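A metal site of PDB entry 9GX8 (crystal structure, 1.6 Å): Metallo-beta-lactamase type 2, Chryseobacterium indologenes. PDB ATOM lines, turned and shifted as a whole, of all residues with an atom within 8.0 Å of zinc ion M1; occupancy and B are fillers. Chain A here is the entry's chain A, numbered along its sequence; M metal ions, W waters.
A ring nitrogen (ND1) of His 213 is in hydrogen-bond range of the backbone carbonyl oxygen (O) of Pro 44, 2.6 Å away.
Zinc ion M1 is bound by water W2, a ring nitrogen (NE2) of His 213, the side-chain carboxylate (OD2) of Asp 94, the side-chain sulfur (SG) of Cys 172 and water W1.
Zinc ion M1 has five donor atoms within binding distance.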
ATOM      1  N   LYS A  35      20.253 -33.422  -2.475  1.00  0.00           N
ATOM      2  CA  LYS A  35      19.844 -33.500  -1.085  1.00  0.00           C
ATOM      3  C   LYS A  35      18.531 -34.254  -1.011  1.00  0.00           C
ATOM      4  O   LYS A  35      17.551 -33.869  -1.655  1.00  0.00           O
ATOM      5  CB  LYS A  35      19.708 -32.096  -0.500  1.00  0.00           C
ATOM      6  CG  LYS A  35      19.106 -32.026   0.884  1.00  0.00           C
ATOM      7  CD  LYS A  35      19.000 -30.576   1.332  1.00  0.00           C
ATOM      8  CE  LYS A  35      18.254 -30.459   2.654  1.00  0.00           C
ATOM      9  NZ  LYS A  35      18.805 -31.324   3.736  1.00  0.00           N
ATOM     10  N   VAL A  43      16.473 -33.379  -4.301  1.00  0.00           N
ATOM     11  CA  VAL A  43      16.536 -31.993  -4.762  1.00  0.00           C
ATOM     12  C   VAL A  43      17.909 -31.713  -5.360  1.00  0.00           C
ATOM     13  O   VAL A  43      18.923 -31.932  -4.682  1.00  0.00           O
ATOM     14  CB  VAL A  43      16.245 -31.017  -3.613  1.00  0.00           C
ATOM     15  CG1 VAL A  43      16.508 -29.585  -4.050  1.00  0.00           C
ATOM     16  CG2 VAL A  43      14.802 -31.176  -3.146  1.00  0.00           C
ATOM     17  N   PRO A  44      18.003 -31.218  -6.591  1.00  0.00           N
ATOM     18  CA  PRO A  44      19.298 -30.786  -7.111  1.00  0.00           C
ATOM     19  C   PRO A  44      19.687 -29.430  -6.544  1.00  0.00           C
ATOM     20  O   PRO A  44      18.851 -28.540  -6.377  1.00  0.00           O
ATOM     21  CB  PRO A  44      19.059 -30.710  -8.624  1.00  0.00           C
ATOM     22  CG  PRO A  44      17.607 -30.375  -8.750  1.00  0.00           C
ATOM     23  CD  PRO A  44      16.916 -31.058  -7.573  1.00  0.00           C
ATOM     24  N   CYS A  45      20.974 -29.297  -6.229  1.00  0.00           N
ATOM     25  CA  CYS A  45      21.521 -28.123  -5.550  1.00  0.00           C
ATOM     26  C   CYS A  45      22.725 -27.609  -6.321  1.00  0.00           C
ATOM     27  O   CYS A  45      23.700 -28.351  -6.502  1.00  0.00           O
ATOM     28  CB  CYS A  45      21.926 -28.462  -4.112  1.00  0.00           C
ATOM     29  SG  CYS A  45      20.607 -29.213  -3.136  1.00  0.00           S
ATOM     30  N   ASN A  46      22.681 -26.343  -6.727  1.00  0.00           N
ATOM     31  CA  ASN A  46      23.691 -25.765  -7.599  1.00  0.00           C
ATOM     32  C   ASN A  46      24.714 -24.929  -6.826  1.00  0.00           C
ATOM     33  O   ASN A  46      24.405 -24.310  -5.797  1.00  0.00           O
ATOM     34  CB  ASN A  46      23.050 -24.863  -8.658  1.00  0.00           C
ATOM     35  CG  ASN A  46      22.097 -25.623  -9.554  1.00  0.00           C
ATOM     36  OD1 ASN A  46      22.314 -26.810  -9.877  1.00  0.00           O
ATOM     37  ND2 ASN A  46      21.048 -24.939 -10.021  1.00  0.00           N
ATOM     38  N   ASP A  60      29.211 -21.777  -3.028  1.00  0.00           N
ATOM     39  CA  ASP A  60      28.494 -22.919  -2.441  1.00  0.00           C
ATOM     40  C   ASP A  60      29.293 -24.205  -2.377  1.00  0.00           C
ATOM     41  O   ASP A  60      29.922 -24.618  -3.356  1.00  0.00           O
ATOM     42  CB  ASP A  60      27.192 -23.175  -3.178  1.00  0.00           C
ATOM     43  CG  ASP A  60      26.072 -22.309  -2.667  1.00  0.00           C
ATOM     44  OD1 ASP A  60      26.382 -21.261  -2.074  1.00  0.00           O
ATOM     45  OD2 ASP A  60      24.891 -22.680  -2.853  1.00  0.00           O
ATOM     46  N   THR A  89      26.855 -19.386   0.122  1.00  0.00           N
ATOM     47  CA  THR A  89      26.015 -18.207  -0.057  1.00  0.00           C
ATOM     48  C   THR A  89      24.883 -18.123   0.952  1.00  0.00           C
ATOM     49  O   THR A  89      24.230 -17.089   1.017  1.00  0.00           O
ATOM     50  CB  THR A  89      25.444 -18.119  -1.480  1.00  0.00           C
ATOM     51  OG1 THR A  89      24.635 -19.268  -1.769  1.00  0.00           O
ATOM     52  CG2 THR A  89      26.570 -18.003  -2.506  1.00  0.00           C
ATOM     53  N   HIS A  90      24.623 -19.179   1.721  1.00  0.00           N
ATOM     54  CA  HIS A  90      23.823 -19.037   2.943  1.00  0.00           C
ATOM     55  C   HIS A  90      24.074 -20.265   3.810  1.00  0.00           C
ATOM     56  O   HIS A  90      24.835 -21.155   3.438  1.00  0.00           O
ATOM     57  CB  HIS A  90      22.345 -18.816   2.639  1.00  0.00           C
ATOM     58  CG  HIS A  90      21.624 -20.019   2.130  1.00  0.00           C
ATOM     59  ND1 HIS A  90      22.027 -20.745   1.024  1.00  0.00           N
ATOM     60  CD2 HIS A  90      20.468 -20.596   2.549  1.00  0.00           C
ATOM     61  CE1 HIS A  90      21.171 -21.725   0.801  1.00  0.00           C
ATOM     62  NE2 HIS A  90      20.214 -21.651   1.713  1.00  0.00           N
ATOM     63  N   HIS A  92      22.260 -22.824   5.022  1.00  0.00           N
ATOM     64  CA  HIS A  92      21.670 -24.146   4.852  1.00  0.00           C
ATOM     65  C   HIS A  92      22.678 -25.123   4.238  1.00  0.00           C
ATOM     66  O   HIS A  92      23.644 -24.725   3.597  1.00  0.00           O
ATOM     67  CB  HIS A  92      20.438 -24.071   3.959  1.00  0.00           C
ATOM     68  CG  HIS A  92      19.274 -23.371   4.590  1.00  0.00           C
ATOM     69  ND1 HIS A  92      18.202 -22.913   3.866  1.00  0.00           N
ATOM     70  CD2 HIS A  92      18.997 -23.097   5.883  1.00  0.00           C
ATOM     71  CE1 HIS A  92      17.315 -22.353   4.674  1.00  0.00           C
ATOM     72  NE2 HIS A  92      17.780 -22.465   5.910  1.00  0.00           N
ATOM     73  N   ASP A  93      22.412 -26.426   4.410  1.00  0.00           N
ATOM     74  CA  ASP A  93      23.405 -27.399   3.993  1.00  0.00           C
ATOM     75  C   ASP A  93      23.567 -27.423   2.485  1.00  0.00           C
ATOM     76  O   ASP A  93      24.631 -27.815   2.014  1.00  0.00           O
ATOM     77  CB  ASP A  93      23.087 -28.815   4.502  1.00  0.00           C
ATOM     78  CG  ASP A  93      21.710 -29.306   4.110  1.00  0.00           C
ATOM     79  OD1 ASP A  93      20.880 -28.501   3.655  1.00  0.00           O
ATOM     80  OD2 ASP A  93      21.464 -30.528   4.262  1.00  0.00           O
ATOM     81  N   ASP A  94      22.569 -26.987   1.710  1.00  0.00           N
ATOM     82  CA  ASP A  94      22.790 -27.044   0.266  1.00  0.00           C
ATOM     83  C   ASP A  94      23.649 -25.890  -0.258  1.00  0.00           C
ATOM     84  O   ASP A  94      23.910 -25.837  -1.460  1.00  0.00           O
ATOM     85  CB  ASP A  94      21.468 -27.100  -0.514  1.00  0.00           C
ATOM     86  CG  ASP A  94      20.519 -25.972  -0.172  1.00  0.00           C
ATOM     87  OD1 ASP A  94      20.219 -25.782   1.028  1.00  0.00           O
ATOM     88  OD2 ASP A  94      20.077 -25.282  -1.106  1.00  0.00           O
ATOM     89  N   SER A  95      24.101 -24.993   0.616  1.00  0.00           N
ATOM     90  CA  SER A  95      25.191 -24.084   0.295  1.00  0.00           C
ATOM     91  C   SER A  95      26.408 -24.249   1.171  1.00  0.00           C
ATOM     92  O   SER A  95      27.497 -23.808   0.775  1.00  0.00           O
ATOM     93  CB  SER A  95      24.752 -22.607   0.377  1.00  0.00           C
ATOM     94  OG  SER A  95      23.705 -22.314  -0.548  1.00  0.00           O
ATOM     95  N   HIS A 153      15.253 -15.546   0.747  1.00  0.00           N
ATOM     96  CA  HIS A 153      15.213 -16.964   1.080  1.00  0.00           C
ATOM     97  C   HIS A 153      15.660 -17.204   2.514  1.00  0.00           C
ATOM     98  O   HIS A 153      15.066 -18.032   3.232  1.00  0.00           O
ATOM     99  CB  HIS A 153      16.092 -17.746   0.102  1.00  0.00           C
ATOM    100  CG  HIS A 153      16.236 -19.175   0.475  1.00  0.00           C
ATOM    101  ND1 HIS A 153      15.211 -20.073   0.349  1.00  0.00           N
ATOM    102  CD2 HIS A 153      17.271 -19.852   1.005  1.00  0.00           C
ATOM    103  CE1 HIS A 153      15.606 -21.255   0.758  1.00  0.00           C
ATOM    104  NE2 HIS A 153      16.853 -21.143   1.179  1.00  0.00           N
ATOM    105  N   THR A 154      16.722 -16.525   2.942  1.00  0.00           N
ATOM    106  CA  THR A 154      17.114 -16.492   4.347  1.00  0.00           C
ATOM    107  C   THR A 154      17.512 -15.061   4.681  1.00  0.00           C
ATOM    108  O   THR A 154      17.528 -14.187   3.814  1.00  0.00           O
ATOM    109  CB  THR A 154      18.277 -17.450   4.646  1.00  0.00           C
ATOM    110  OG1 THR A 154      19.331 -17.203   3.707  1.00  0.00           O
ATOM    111  CG2 THR A 154      17.830 -18.915   4.585  1.00  0.00           C
ATOM    112  N   GLY A 171      22.209 -18.077  -6.006  1.00  0.00           N
ATOM    113  CA  GLY A 171      21.975 -18.918  -4.853  1.00  0.00           C
ATOM    114  C   GLY A 171      20.478 -19.148  -4.661  1.00  0.00           C
ATOM    115  O   GLY A 171      19.664 -18.995  -5.573  1.00  0.00           O
ATOM    116  N   CYS A 172      20.115 -19.486  -3.424  1.00  0.00           N
ATOM    117  CA  CYS A 172      18.721 -19.858  -3.204  1.00  0.00           C
ATOM    118  C   CYS A 172      17.789 -18.654  -3.122  1.00  0.00           C
ATOM    119  O   CYS A 172      16.578 -18.827  -3.063  1.00  0.00           O
ATOM    120  CB  CYS A 172      18.622 -20.733  -1.977  1.00  0.00           C
ATOM    121  SG  CYS A 172      19.482 -22.290  -2.256  1.00  0.00           S
ATOM    122  N   LEU A 173      18.344 -17.443  -3.141  1.00  0.00           N
ATOM    123  CA  LEU A 173      17.557 -16.239  -3.338  1.00  0.00           C
ATOM    124  C   LEU A 173      16.898 -16.208  -4.704  1.00  0.00           C
ATOM    125  O   LEU A 173      15.865 -15.540  -4.882  1.00  0.00           O
ATOM    126  CB  LEU A 173      18.468 -15.016  -3.161  1.00  0.00           C
ATOM    127  CG  LEU A 173      17.815 -13.656  -3.366  1.00  0.00           C
ATOM    128  CD1 LEU A 173      16.994 -13.315  -2.119  1.00  0.00           C
ATOM    129  CD2 LEU A 173      18.881 -12.591  -3.607  1.00  0.00           C
ATOM    130  N   LEU A 174      17.478 -16.890  -5.689  1.00  0.00           N
ATOM    131  CA  LEU A 174      16.950 -16.922  -7.035  1.00  0.00           C
ATOM    132  C   LEU A 174      16.245 -18.242  -7.297  1.00  0.00           C
ATOM    133  O   LEU A 174      16.775 -19.313  -6.978  1.00  0.00           O
ATOM    134  CB  LEU A 174      18.064 -16.720  -8.061  1.00  0.00           C
ATOM    135  CG  LEU A 174      18.349 -15.271  -8.482  1.00  0.00           C
ATOM    136  CD1 LEU A 174      17.190 -14.712  -9.328  1.00  0.00           C
ATOM    137  CD2 LEU A 174      18.621 -14.412  -7.252  1.00  0.00           C
ATOM    138  N   LYS A 175      15.069 -18.169  -7.902  1.00  0.00           N
ATOM    139  CA  LYS A 175      14.306 -19.342  -8.326  1.00  0.00           C
ATOM    140  C   LYS A 175      14.504 -19.615  -9.811  1.00  0.00           C
ATOM    141  O   LYS A 175      14.665 -18.689 -10.603  1.00  0.00           O
ATOM    142  CB  LYS A 175      12.817 -19.148  -8.060  1.00  0.00           C
ATOM    143  CG  LYS A 175      12.458 -19.009  -6.576  1.00  0.00           C
ATOM    144  CD  LYS A 175      12.844 -20.263  -5.806  1.00  0.00           C
ATOM    145  CE  LYS A 175      12.367 -20.165  -4.357  1.00  0.00           C
ATOM    146  NZ  LYS A 175      12.761 -21.392  -3.576  1.00  0.00           N
ATOM    147  N   TYR A 183      11.068 -23.812   0.381  1.00  0.00           N
ATOM    148  CA  TYR A 183      11.081 -23.818   1.843  1.00  0.00           C
ATOM    149  C   TYR A 183      11.160 -22.391   2.375  1.00  0.00           C
ATOM    150  O   TYR A 183      12.113 -21.661   2.066  1.00  0.00           O
ATOM    151  CB  TYR A 183      12.261 -24.646   2.363  1.00  0.00           C
ATOM    152  CG  TYR A 183      12.406 -24.591   3.864  1.00  0.00           C
ATOM    153  CD1 TYR A 183      13.500 -23.963   4.451  1.00  0.00           C
ATOM    154  CD2 TYR A 183      11.449 -25.152   4.695  1.00  0.00           C
ATOM    155  CE1 TYR A 183      13.628 -23.902   5.834  1.00  0.00           C
ATOM    156  CE2 TYR A 183      11.564 -25.104   6.067  1.00  0.00           C
ATOM    157  CZ  TYR A 183      12.653 -24.479   6.636  1.00  0.00           C
ATOM    158  OH  TYR A 183      12.742 -24.456   8.013  1.00  0.00           O
ATOM    159  N   PRO A 211      20.171 -20.250 -10.413  1.00  0.00           N
ATOM    160  CA  PRO A 211      19.408 -20.388  -9.168  1.00  0.00           C
ATOM    161  C   PRO A 211      20.020 -21.465  -8.277  1.00  0.00           C
ATOM    162  O   PRO A 211      20.816 -22.294  -8.717  1.00  0.00           O
ATOM    163  CB  PRO A 211      18.030 -20.835  -9.671  1.00  0.00           C
ATOM    164  CG  PRO A 211      18.389 -21.707 -10.874  1.00  0.00           C
ATOM    165  CD  PRO A 211      19.583 -21.034 -11.507  1.00  0.00           C
ATOM    166  N   GLY A 212      19.617 -21.428  -6.999  1.00  0.00           N
ATOM    167  CA  GLY A 212      20.111 -22.441  -6.070  1.00  0.00           C
ATOM    168  C   GLY A 212      19.659 -23.839  -6.414  1.00  0.00           C
ATOM    169  O   GLY A 212      20.338 -24.815  -6.078  1.00  0.00           O
ATOM    170  N   HIS A 213      18.522 -23.962  -7.097  1.00  0.00           N
ATOM    171  CA  HIS A 213      17.977 -25.255  -7.489  1.00  0.00           C
ATOM    172  C   HIS A 213      17.401 -25.151  -8.883  1.00  0.00           C
ATOM    173  O   HIS A 213      16.611 -24.241  -9.155  1.00  0.00           O
ATOM    174  CB  HIS A 213      16.868 -25.719  -6.534  1.00  0.00           C
ATOM    175  CG  HIS A 213      17.294 -25.755  -5.113  1.00  0.00           C
ATOM    176  ND1 HIS A 213      18.086 -26.767  -4.606  1.00  0.00           N
ATOM    177  CD2 HIS A 213      17.076 -24.906  -4.087  1.00  0.00           C
ATOM    178  CE1 HIS A 213      18.312 -26.549  -3.323  1.00  0.00           C
ATOM    179  NE2 HIS A 213      17.708 -25.429  -2.984  1.00  0.00           N
HETATM  180 ZN    ZN M   1      18.249 -23.977  -1.360  1.00  0.00          ZN
HETATM  181 ZN    ZN M   2      18.310 -22.647   1.710  1.00  0.00          ZN
HETATM  182  O   HOH W   1      16.141 -23.134  -1.552  1.00  0.00           O
HETATM  183  O   HOH W   2      17.848 -24.163   0.700  1.00  0.00           O
